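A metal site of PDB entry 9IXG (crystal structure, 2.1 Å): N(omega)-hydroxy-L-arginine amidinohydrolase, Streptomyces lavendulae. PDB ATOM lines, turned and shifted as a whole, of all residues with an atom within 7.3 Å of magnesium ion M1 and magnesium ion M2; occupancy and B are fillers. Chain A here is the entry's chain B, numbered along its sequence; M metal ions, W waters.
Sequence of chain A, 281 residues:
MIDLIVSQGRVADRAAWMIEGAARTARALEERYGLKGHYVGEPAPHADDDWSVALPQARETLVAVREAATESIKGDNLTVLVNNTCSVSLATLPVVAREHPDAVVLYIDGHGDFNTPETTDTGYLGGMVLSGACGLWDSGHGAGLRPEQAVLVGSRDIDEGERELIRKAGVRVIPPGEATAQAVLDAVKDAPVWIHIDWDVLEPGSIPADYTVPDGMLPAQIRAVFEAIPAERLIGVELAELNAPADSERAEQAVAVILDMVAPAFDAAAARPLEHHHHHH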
ATOM      1  N   MET A  18      12.176  18.297  14.867  1.00  0.00           N
ATOM      2  CA  MET A  18      12.592  18.321  16.260  1.00  0.00           C
ATOM      3  C   MET A  18      11.415  18.577  17.194  1.00  0.00           C
ATOM      4  O   MET A  18      11.421  18.078  18.331  1.00  0.00           O
ATOM      5  CB  MET A  18      13.726  19.334  16.428  1.00  0.00           C
ATOM      6  CG  MET A  18      15.086  18.743  15.935  1.00  0.00           C
ATOM      7  SD  MET A  18      16.507  19.796  16.181  1.00  0.00           S
ATOM      8  CE  MET A  18      15.886  21.222  15.288  1.00  0.00           C
ATOM      9  N   THR A  85      14.477  22.053  20.822  1.00  0.00           N
ATOM     10  CA  THR A  85      15.845  22.512  20.594  1.00  0.00           C
ATOM     11  C   THR A  85      16.523  22.913  21.903  1.00  0.00           C
ATOM     12  O   THR A  85      15.853  23.263  22.882  1.00  0.00           O
ATOM     13  CB  THR A  85      15.908  23.704  19.616  1.00  0.00           C
ATOM     14  OG1 THR A  85      15.185  24.813  20.169  1.00  0.00           O
ATOM     15  CG2 THR A  85      15.306  23.343  18.264  1.00  0.00           C
ATOM     16  N   CYS A  86      17.870  22.888  21.893  1.00  0.00           N
ATOM     17  CA  CYS A  86      18.645  23.386  23.031  1.00  0.00           C
ATOM     18  C   CYS A  86      18.332  24.856  23.345  1.00  0.00           C
ATOM     19  O   CYS A  86      18.530  25.295  24.483  1.00  0.00           O
ATOM     20  CB  CYS A  86      20.156  23.247  22.786  1.00  0.00           C
ATOM     21  SG  CYS A  86      20.992  21.605  23.109  1.00  0.00           S
ATOM     22  N   SER A  87      17.865  25.621  22.371  1.00  0.00           N
ATOM     23  CA  SER A  87      17.679  27.059  22.612  1.00  0.00           C
ATOM     24  C   SER A  87      16.571  27.339  23.609  1.00  0.00           C
ATOM     25  O   SER A  87      16.519  28.441  24.163  1.00  0.00           O
ATOM     26  CB  SER A  87      17.391  27.789  21.292  1.00  0.00           C
ATOM     27  OG  SER A  87      18.450  27.598  20.363  1.00  0.00           O
ATOM     28  N   TYR A 107      26.151  19.857  31.127  1.00  0.00           N
ATOM     29  CA  TYR A 107      25.723  20.215  29.782  1.00  0.00           C
ATOM     30  C   TYR A 107      26.313  19.159  28.869  1.00  0.00           C
ATOM     31  O   TYR A 107      27.444  19.296  28.388  1.00  0.00           O
ATOM     32  CB  TYR A 107      26.163  21.635  29.411  1.00  0.00           C
ATOM     33  CG  TYR A 107      25.379  22.216  28.271  1.00  0.00           C
ATOM     34  CD1 TYR A 107      25.749  21.955  26.955  1.00  0.00           C
ATOM     35  CD2 TYR A 107      24.293  23.035  28.500  1.00  0.00           C
ATOM     36  CE1 TYR A 107      25.027  22.491  25.892  1.00  0.00           C
ATOM     37  CE2 TYR A 107      23.556  23.571  27.454  1.00  0.00           C
ATOM     38  CZ  TYR A 107      23.931  23.298  26.153  1.00  0.00           C
ATOM     39  OH  TYR A 107      23.217  23.834  25.127  1.00  0.00           O
ATOM     40  N   ILE A 108      25.546  18.112  28.625  1.00  0.00           N
ATOM     41  CA  ILE A 108      26.006  16.928  27.908  1.00  0.00           C
ATOM     42  C   ILE A 108      25.686  17.123  26.436  1.00  0.00           C
ATOM     43  O   ILE A 108      24.526  17.079  26.007  1.00  0.00           O
ATOM     44  CB  ILE A 108      25.359  15.659  28.478  1.00  0.00           C
ATOM     45  CG1 ILE A 108      25.472  15.668  30.007  1.00  0.00           C
ATOM     46  CG2 ILE A 108      26.037  14.438  27.916  1.00  0.00           C
ATOM     47  CD1 ILE A 108      25.044  14.378  30.679  1.00  0.00           C
ATOM     48  N   ASP A 109      26.729  17.361  25.644  1.00  0.00           N
ATOM     49  CA  ASP A 109      26.560  17.977  24.333  1.00  0.00           C
ATOM     50  C   ASP A 109      27.783  17.681  23.485  1.00  0.00           C
ATOM     51  O   ASP A 109      28.906  17.708  23.988  1.00  0.00           O
ATOM     52  CB  ASP A 109      26.348  19.489  24.522  1.00  0.00           C
ATOM     53  CG  ASP A 109      25.913  20.198  23.253  1.00  0.00           C
ATOM     54  OD1 ASP A 109      26.789  20.654  22.492  1.00  0.00           O
ATOM     55  OD2 ASP A 109      24.669  20.318  23.062  1.00  0.00           O
ATOM     56  N   GLY A 110      27.573  17.376  22.195  1.00  0.00           N
ATOM     57  CA  GLY A 110      28.711  17.152  21.322  1.00  0.00           C
ATOM     58  C   GLY A 110      29.491  18.394  20.900  1.00  0.00           C
ATOM     59  O   GLY A 110      30.602  18.266  20.365  1.00  0.00           O
ATOM     60  N   HIS A 111      28.959  19.592  21.134  1.00  0.00           N
ATOM     61  CA  HIS A 111      29.542  20.805  20.553  1.00  0.00           C
ATOM     62  C   HIS A 111      30.067  21.802  21.560  1.00  0.00           C
ATOM     63  O   HIS A 111      31.093  22.443  21.309  1.00  0.00           O
ATOM     64  CB  HIS A 111      28.513  21.521  19.661  1.00  0.00           C
ATOM     65  CG  HIS A 111      28.209  20.776  18.411  1.00  0.00           C
ATOM     66  ND1 HIS A 111      28.947  20.933  17.257  1.00  0.00           N
ATOM     67  CD2 HIS A 111      27.268  19.846  18.123  1.00  0.00           C
ATOM     68  CE1 HIS A 111      28.464  20.152  16.312  1.00  0.00           C
ATOM     69  NE2 HIS A 111      27.445  19.473  16.815  1.00  0.00           N
ATOM     70  N   GLY A 112      29.372  22.014  22.673  1.00  0.00           N
ATOM     71  CA  GLY A 112      29.729  23.045  23.636  1.00  0.00           C
ATOM     72  C   GLY A 112      28.769  24.214  23.685  1.00  0.00           C
ATOM     73  O   GLY A 112      28.587  24.809  24.751  1.00  0.00           O
ATOM     74  N   ASP A 113      28.179  24.586  22.537  1.00  0.00           N
ATOM     75  CA  ASP A 113      27.125  25.622  22.485  1.00  0.00           C
ATOM     76  C   ASP A 113      27.541  26.906  23.213  1.00  0.00           C
ATOM     77  O   ASP A 113      26.761  27.523  23.949  1.00  0.00           O
ATOM     78  CB  ASP A 113      25.803  25.077  23.046  1.00  0.00           C
ATOM     79  CG  ASP A 113      25.242  23.930  22.205  1.00  0.00           C
ATOM     80  OD1 ASP A 113      25.678  23.801  21.048  1.00  0.00           O
ATOM     81  OD2 ASP A 113      24.360  23.192  22.690  1.00  0.00           O
ATOM     82  N   TYR A 124      23.669  30.254  14.325  1.00  0.00           N
ATOM     83  CA  TYR A 124      22.700  29.363  14.950  1.00  0.00           C
ATOM     84  C   TYR A 124      22.594  29.631  16.454  1.00  0.00           C
ATOM     85  O   TYR A 124      23.532  29.386  17.214  1.00  0.00           O
ATOM     86  CB  TYR A 124      23.070  27.908  14.682  1.00  0.00           C
ATOM     87  CG  TYR A 124      22.061  26.924  15.234  1.00  0.00           C
ATOM     88  CD1 TYR A 124      20.704  27.146  15.074  1.00  0.00           C
ATOM     89  CD2 TYR A 124      22.468  25.766  15.889  1.00  0.00           C
ATOM     90  CE1 TYR A 124      19.769  26.250  15.570  1.00  0.00           C
ATOM     91  CE2 TYR A 124      21.536  24.860  16.375  1.00  0.00           C
ATOM     92  CZ  TYR A 124      20.189  25.120  16.229  1.00  0.00           C
ATOM     93  OH  TYR A 124      19.226  24.242  16.706  1.00  0.00           O
ATOM     94  N   GLY A 126      21.101  27.894  18.575  1.00  0.00           N
ATOM     95  CA  GLY A 126      21.343  26.654  19.291  1.00  0.00           C
ATOM     96  C   GLY A 126      22.787  26.463  19.694  1.00  0.00           C
ATOM     97  O   GLY A 126      23.073  25.702  20.644  1.00  0.00           O
ATOM     98  N   GLY A 127      23.714  27.113  19.002  1.00  0.00           N
ATOM     99  CA  GLY A 127      25.094  27.119  19.418  1.00  0.00           C
ATOM    100  C   GLY A 127      25.487  28.223  20.375  1.00  0.00           C
ATOM    101  O   GLY A 127      26.677  28.409  20.634  1.00  0.00           O
ATOM    102  N   VAL A 129      23.723  28.766  23.554  1.00  0.00           N
ATOM    103  CA  VAL A 129      22.818  28.574  24.689  1.00  0.00           C
ATOM    104  C   VAL A 129      23.563  28.703  26.018  1.00  0.00           C
ATOM    105  O   VAL A 129      23.151  29.460  26.911  1.00  0.00           O
ATOM    106  CB  VAL A 129      22.115  27.205  24.581  1.00  0.00           C
ATOM    107  CG1 VAL A 129      21.427  26.797  25.903  1.00  0.00           C
ATOM    108  CG2 VAL A 129      21.144  27.216  23.421  1.00  0.00           C
ATOM    109  N   HIS A 196      21.439  18.607  31.354  1.00  0.00           N
ATOM    110  CA  HIS A 196      20.981  18.991  30.025  1.00  0.00           C
ATOM    111  C   HIS A 196      21.638  18.041  29.033  1.00  0.00           C
ATOM    112  O   HIS A 196      22.864  17.910  29.028  1.00  0.00           O
ATOM    113  CB  HIS A 196      21.360  20.446  29.736  1.00  0.00           C
ATOM    114  CG  HIS A 196      21.157  20.858  28.306  1.00  0.00           C
ATOM    115  ND1 HIS A 196      20.224  21.791  27.936  1.00  0.00           N
ATOM    116  CD2 HIS A 196      21.784  20.468  27.167  1.00  0.00           C
ATOM    117  CE1 HIS A 196      20.273  21.967  26.616  1.00  0.00           C
ATOM    118  NE2 HIS A 196      21.208  21.171  26.126  1.00  0.00           N
ATOM    119  N   ILE A 197      20.867  17.359  28.217  1.00  0.00           N
ATOM    120  CA  ILE A 197      21.476  16.466  27.230  1.00  0.00           C
ATOM    121  C   ILE A 197      20.942  16.757  25.826  1.00  0.00           C
ATOM    122  O   ILE A 197      19.723  16.820  25.610  1.00  0.00           O
ATOM    123  CB  ILE A 197      21.303  14.981  27.605  1.00  0.00           C
ATOM    124  CG1 ILE A 197      22.060  14.088  26.603  1.00  0.00           C
ATOM    125  CG2 ILE A 197      19.852  14.605  27.739  1.00  0.00           C
ATOM    126  CD1 ILE A 197      22.477  12.779  27.204  1.00  0.00           C
ATOM    127  N   ASP A 198      21.862  16.947  24.890  1.00  0.00           N
ATOM    128  CA  ASP A 198      21.606  17.086  23.461  1.00  0.00           C
ATOM    129  C   ASP A 198      22.096  15.792  22.807  1.00  0.00           C
ATOM    130  O   ASP A 198      23.254  15.408  22.977  1.00  0.00           O
ATOM    131  CB  ASP A 198      22.335  18.336  22.944  1.00  0.00           C
ATOM    132  CG  ASP A 198      22.273  18.513  21.426  1.00  0.00           C
ATOM    133  OD1 ASP A 198      21.808  17.628  20.667  1.00  0.00           O
ATOM    134  OD2 ASP A 198      22.711  19.591  20.976  1.00  0.00           O
ATOM    135  N   TRP A 199      21.188  15.087  22.128  1.00  0.00           N
ATOM    136  CA  TRP A 199      21.528  13.766  21.611  1.00  0.00           C
ATOM    137  C   TRP A 199      22.668  13.776  20.607  1.00  0.00           C
ATOM    138  O   TRP A 199      23.145  12.690  20.242  1.00  0.00           O
ATOM    139  CB  TRP A 199      20.284  13.117  21.005  1.00  0.00           C
ATOM    140  CG  TRP A 199      19.189  13.036  22.008  1.00  0.00           C
ATOM    141  CD1 TRP A 199      17.924  13.576  21.908  1.00  0.00           C
ATOM    142  CD2 TRP A 199      19.271  12.436  23.304  1.00  0.00           C
ATOM    143  NE1 TRP A 199      17.213  13.312  23.051  1.00  0.00           N
ATOM    144  CE2 TRP A 199      18.006  12.612  23.918  1.00  0.00           C
ATOM    145  CE3 TRP A 199      20.267  11.729  23.981  1.00  0.00           C
ATOM    146  CZ2 TRP A 199      17.727  12.132  25.201  1.00  0.00           C
ATOM    147  CZ3 TRP A 199      19.984  11.242  25.259  1.00  0.00           C
ATOM    148  CH2 TRP A 199      18.720  11.456  25.851  1.00  0.00           C
ATOM    149  N   ASP A 200      23.143  14.944  20.164  1.00  0.00           N
ATOM    150  CA  ASP A 200      24.319  14.974  19.318  1.00  0.00           C
ATOM    151  C   ASP A 200      25.593  14.566  20.054  1.00  0.00           C
ATOM    152  O   ASP A 200      26.597  14.272  19.397  1.00  0.00           O
ATOM    153  CB  ASP A 200      24.455  16.359  18.620  1.00  0.00           C
ATOM    154  CG  ASP A 200      24.765  17.534  19.577  1.00  0.00           C
ATOM    155  OD1 ASP A 200      25.397  17.365  20.622  1.00  0.00           O
ATOM    156  OD2 ASP A 200      24.394  18.683  19.227  1.00  0.00           O
ATOM    157  N   VAL A 201      25.581  14.504  21.386  1.00  0.00           N
ATOM    158  CA  VAL A 201      26.722  13.979  22.135  1.00  0.00           C
ATOM    159  C   VAL A 201      27.020  12.529  21.801  1.00  0.00           C
ATOM    160  O   VAL A 201      28.151  12.072  22.014  1.00  0.00           O
ATOM    161  CB  VAL A 201      26.481  14.159  23.649  1.00  0.00           C
ATOM    162  CG1 VAL A 201      25.471  13.110  24.177  1.00  0.00           C
ATOM    163  CG2 VAL A 201      27.788  14.106  24.426  1.00  0.00           C
ATOM    164  N   ALA A 209      20.065  13.059  15.021  1.00  0.00           N
ATOM    165  CA  ALA A 209      20.168  14.451  15.442  1.00  0.00           C
ATOM    166  C   ALA A 209      20.915  15.226  14.369  1.00  0.00           C
ATOM    167  O   ALA A 209      21.807  14.684  13.696  1.00  0.00           O
ATOM    168  CB  ALA A 209      20.890  14.583  16.793  1.00  0.00           C
ATOM    169  N   ASP A 210      20.574  16.507  14.200  1.00  0.00           N
ATOM    170  CA  ASP A 210      21.381  17.344  13.323  1.00  0.00           C
ATOM    171  C   ASP A 210      22.681  17.718  14.040  1.00  0.00           C
ATOM    172  O   ASP A 210      22.856  17.506  15.245  1.00  0.00           O
ATOM    173  CB  ASP A 210      20.597  18.586  12.864  1.00  0.00           C
ATOM    174  CG  ASP A 210      20.163  19.506  14.016  1.00  0.00           C
ATOM    175  OD1 ASP A 210      20.193  19.073  15.195  1.00  0.00           O
ATOM    176  OD2 ASP A 210      19.788  20.674  13.733  1.00  0.00           O
ATOM    177  N   TYR A 211      23.640  18.238  13.254  1.00  0.00           N
ATOM    178  CA  TYR A 211      24.949  18.658  13.785  1.00  0.00           C
ATOM    179  C   TYR A 211      25.698  17.472  14.425  1.00  0.00           C
ATOM    180  O   TYR A 211      26.226  17.563  15.542  1.00  0.00           O
ATOM    181  CB  TYR A 211      24.782  19.815  14.784  1.00  0.00           C
ATOM    182  CG  TYR A 211      24.341  21.125  14.139  1.00  0.00           C
ATOM    183  CD1 TYR A 211      25.257  21.923  13.460  1.00  0.00           C
ATOM    184  CD2 TYR A 211      23.017  21.567  14.214  1.00  0.00           C
ATOM    185  CE1 TYR A 211      24.874  23.133  12.876  1.00  0.00           C
ATOM    186  CE2 TYR A 211      22.620  22.772  13.631  1.00  0.00           C
ATOM    187  CZ  TYR A 211      23.559  23.546  12.965  1.00  0.00           C
ATOM    188  OH  TYR A 211      23.194  24.743  12.380  1.00  0.00           O
ATOM    189  N   THR A 212      25.728  16.350  13.696  1.00  0.00           N
ATOM    190  CA  THR A 212      26.417  15.123  14.104  1.00  0.00           C
ATOM    191  C   THR A 212      27.929  15.349  14.136  1.00  0.00           C
ATOM    192  O   THR A 212      28.478  16.098  13.328  1.00  0.00           O
ATOM    193  CB  THR A 212      26.076  13.995  13.126  1.00  0.00           C
ATOM    194  OG1 THR A 212      24.663  13.743  13.138  1.00  0.00           O
ATOM    195  CG2 THR A 212      26.768  12.730  13.479  1.00  0.00           C
ATOM    196  N   ALA A 240      16.779  16.970  24.644  1.00  0.00           N
ATOM    197  CA  ALA A 240      16.638  17.857  23.505  1.00  0.00           C
ATOM    198  C   ALA A 240      17.191  17.245  22.231  1.00  0.00           C
ATOM    199  O   ALA A 240      18.233  16.565  22.261  1.00  0.00           O
ATOM    200  CB  ALA A 240      17.351  19.209  23.751  1.00  0.00           C
ATOM    201  N   GLU A 241      16.494  17.518  21.129  1.00  0.00           N
ATOM    202  CA  GLU A 241      17.007  17.520  19.741  1.00  0.00           C
ATOM    203  C   GLU A 241      16.956  16.149  19.077  1.00  0.00           C
ATOM    204  O   GLU A 241      17.865  15.795  18.311  1.00  0.00           O
ATOM    205  CB  GLU A 241      18.431  18.096  19.664  1.00  0.00           C
ATOM    206  CG  GLU A 241      18.562  19.470  20.320  1.00  0.00           C
ATOM    207  CD  GLU A 241      19.371  20.448  19.524  1.00  0.00           C
ATOM    208  OE1 GLU A 241      19.071  21.671  19.596  1.00  0.00           O
ATOM    209  OE2 GLU A 241      20.326  20.006  18.833  1.00  0.00           O
HETATM  210 MG    MG M   1      23.391  21.537  21.822  1.00  0.00          MG
HETATM  211 MG    MG M   2      22.240  19.214  18.946  1.00  0.00          MG
HETATM  212  O   HOH W   1      21.528  17.945  17.271  1.00  0.00           O
HETATM  213  O   HOH W   2      22.584  21.053  18.211  1.00  0.00           O
HETATM  214  O   HOH W   3      22.307  22.955  20.539  1.00  0.00           O
HETATM  215  O   HOH W   4      24.924  21.031  20.163  1.00  0.00           O
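Water W4 lies within hydrogen-bond range of OD1 of Asp 113 (3.0 Å) and OD1 of Asp 109 (3.0 Å).
Magnesium ion M1 is bound by OD2 of Asp 113 (2.1 Å), OD2 of Asp 109 (2.2 Å), water W3 (2.2 Å), OD2 of Asp 198 (2.2 Å), water W4 (2.3 Å) and SG of Cys 86 (2.7 Å).
Magnesium ion M1 has six donor atoms within binding distance.
Of the 27 residues printed, 3 come within 4 Å of magnesium ion M2.
Along chain A the residues within 4 Å of magnesium ion M2 span positions 198 to 241.
Magnesium ion M2 is bound by water W2 (2.0 Å), OE2 of Glu 241 (2.1 Å), OD2 of Asp 198 (2.1 Å), water W1 (2.2 Å), OD2 of Asp 200 (2.2 Å) and OD1 of Asp 198 (2.4 Å).
Magnesium ion M2 has six donor atoms within binding distance.
A ring nitrogen (NE2) of His 196 sits close to the side-chain sulfur of Cys 86 (3.1 Å).
OD1 of Asp 200 is in hydrogen-bond range of N of Gly 110, at 2.7 Å.
The backbone NH of His 111 lies within hydrogen-bond range of the side-chain carboxylate of Asp 109, 2.8 Å away.
The backbone NH (N) of Asp 198 lies within hydrogen-bond range of the backbone carbonyl oxygen (O) of Ile 108 (2.9 Å).
The side-chain sulfur (SG) of Cys 86 sits close to the side-chain hydroxyl (OH) of Tyr 107, at 3.7 Å.
N of Val 129 sits at hydrogen-bond distance from O of Asp 113 (3.3 Å).
The backbone NH (N) of Gly 112 is in hydrogen-bond range of the side-chain carboxylate (OD1) of Asp 109, at 2.9 Å.
OH of Tyr 107 sits close to OD2 of Asp 113.
Within 4 Å of magnesium ion M1: Cys 86, Asp 109, Asp 113, Asp 198 and Asp 200.
The nearest printed residue that does not touch magnesium ion M1 is Tyr 107 (4.03 Å).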
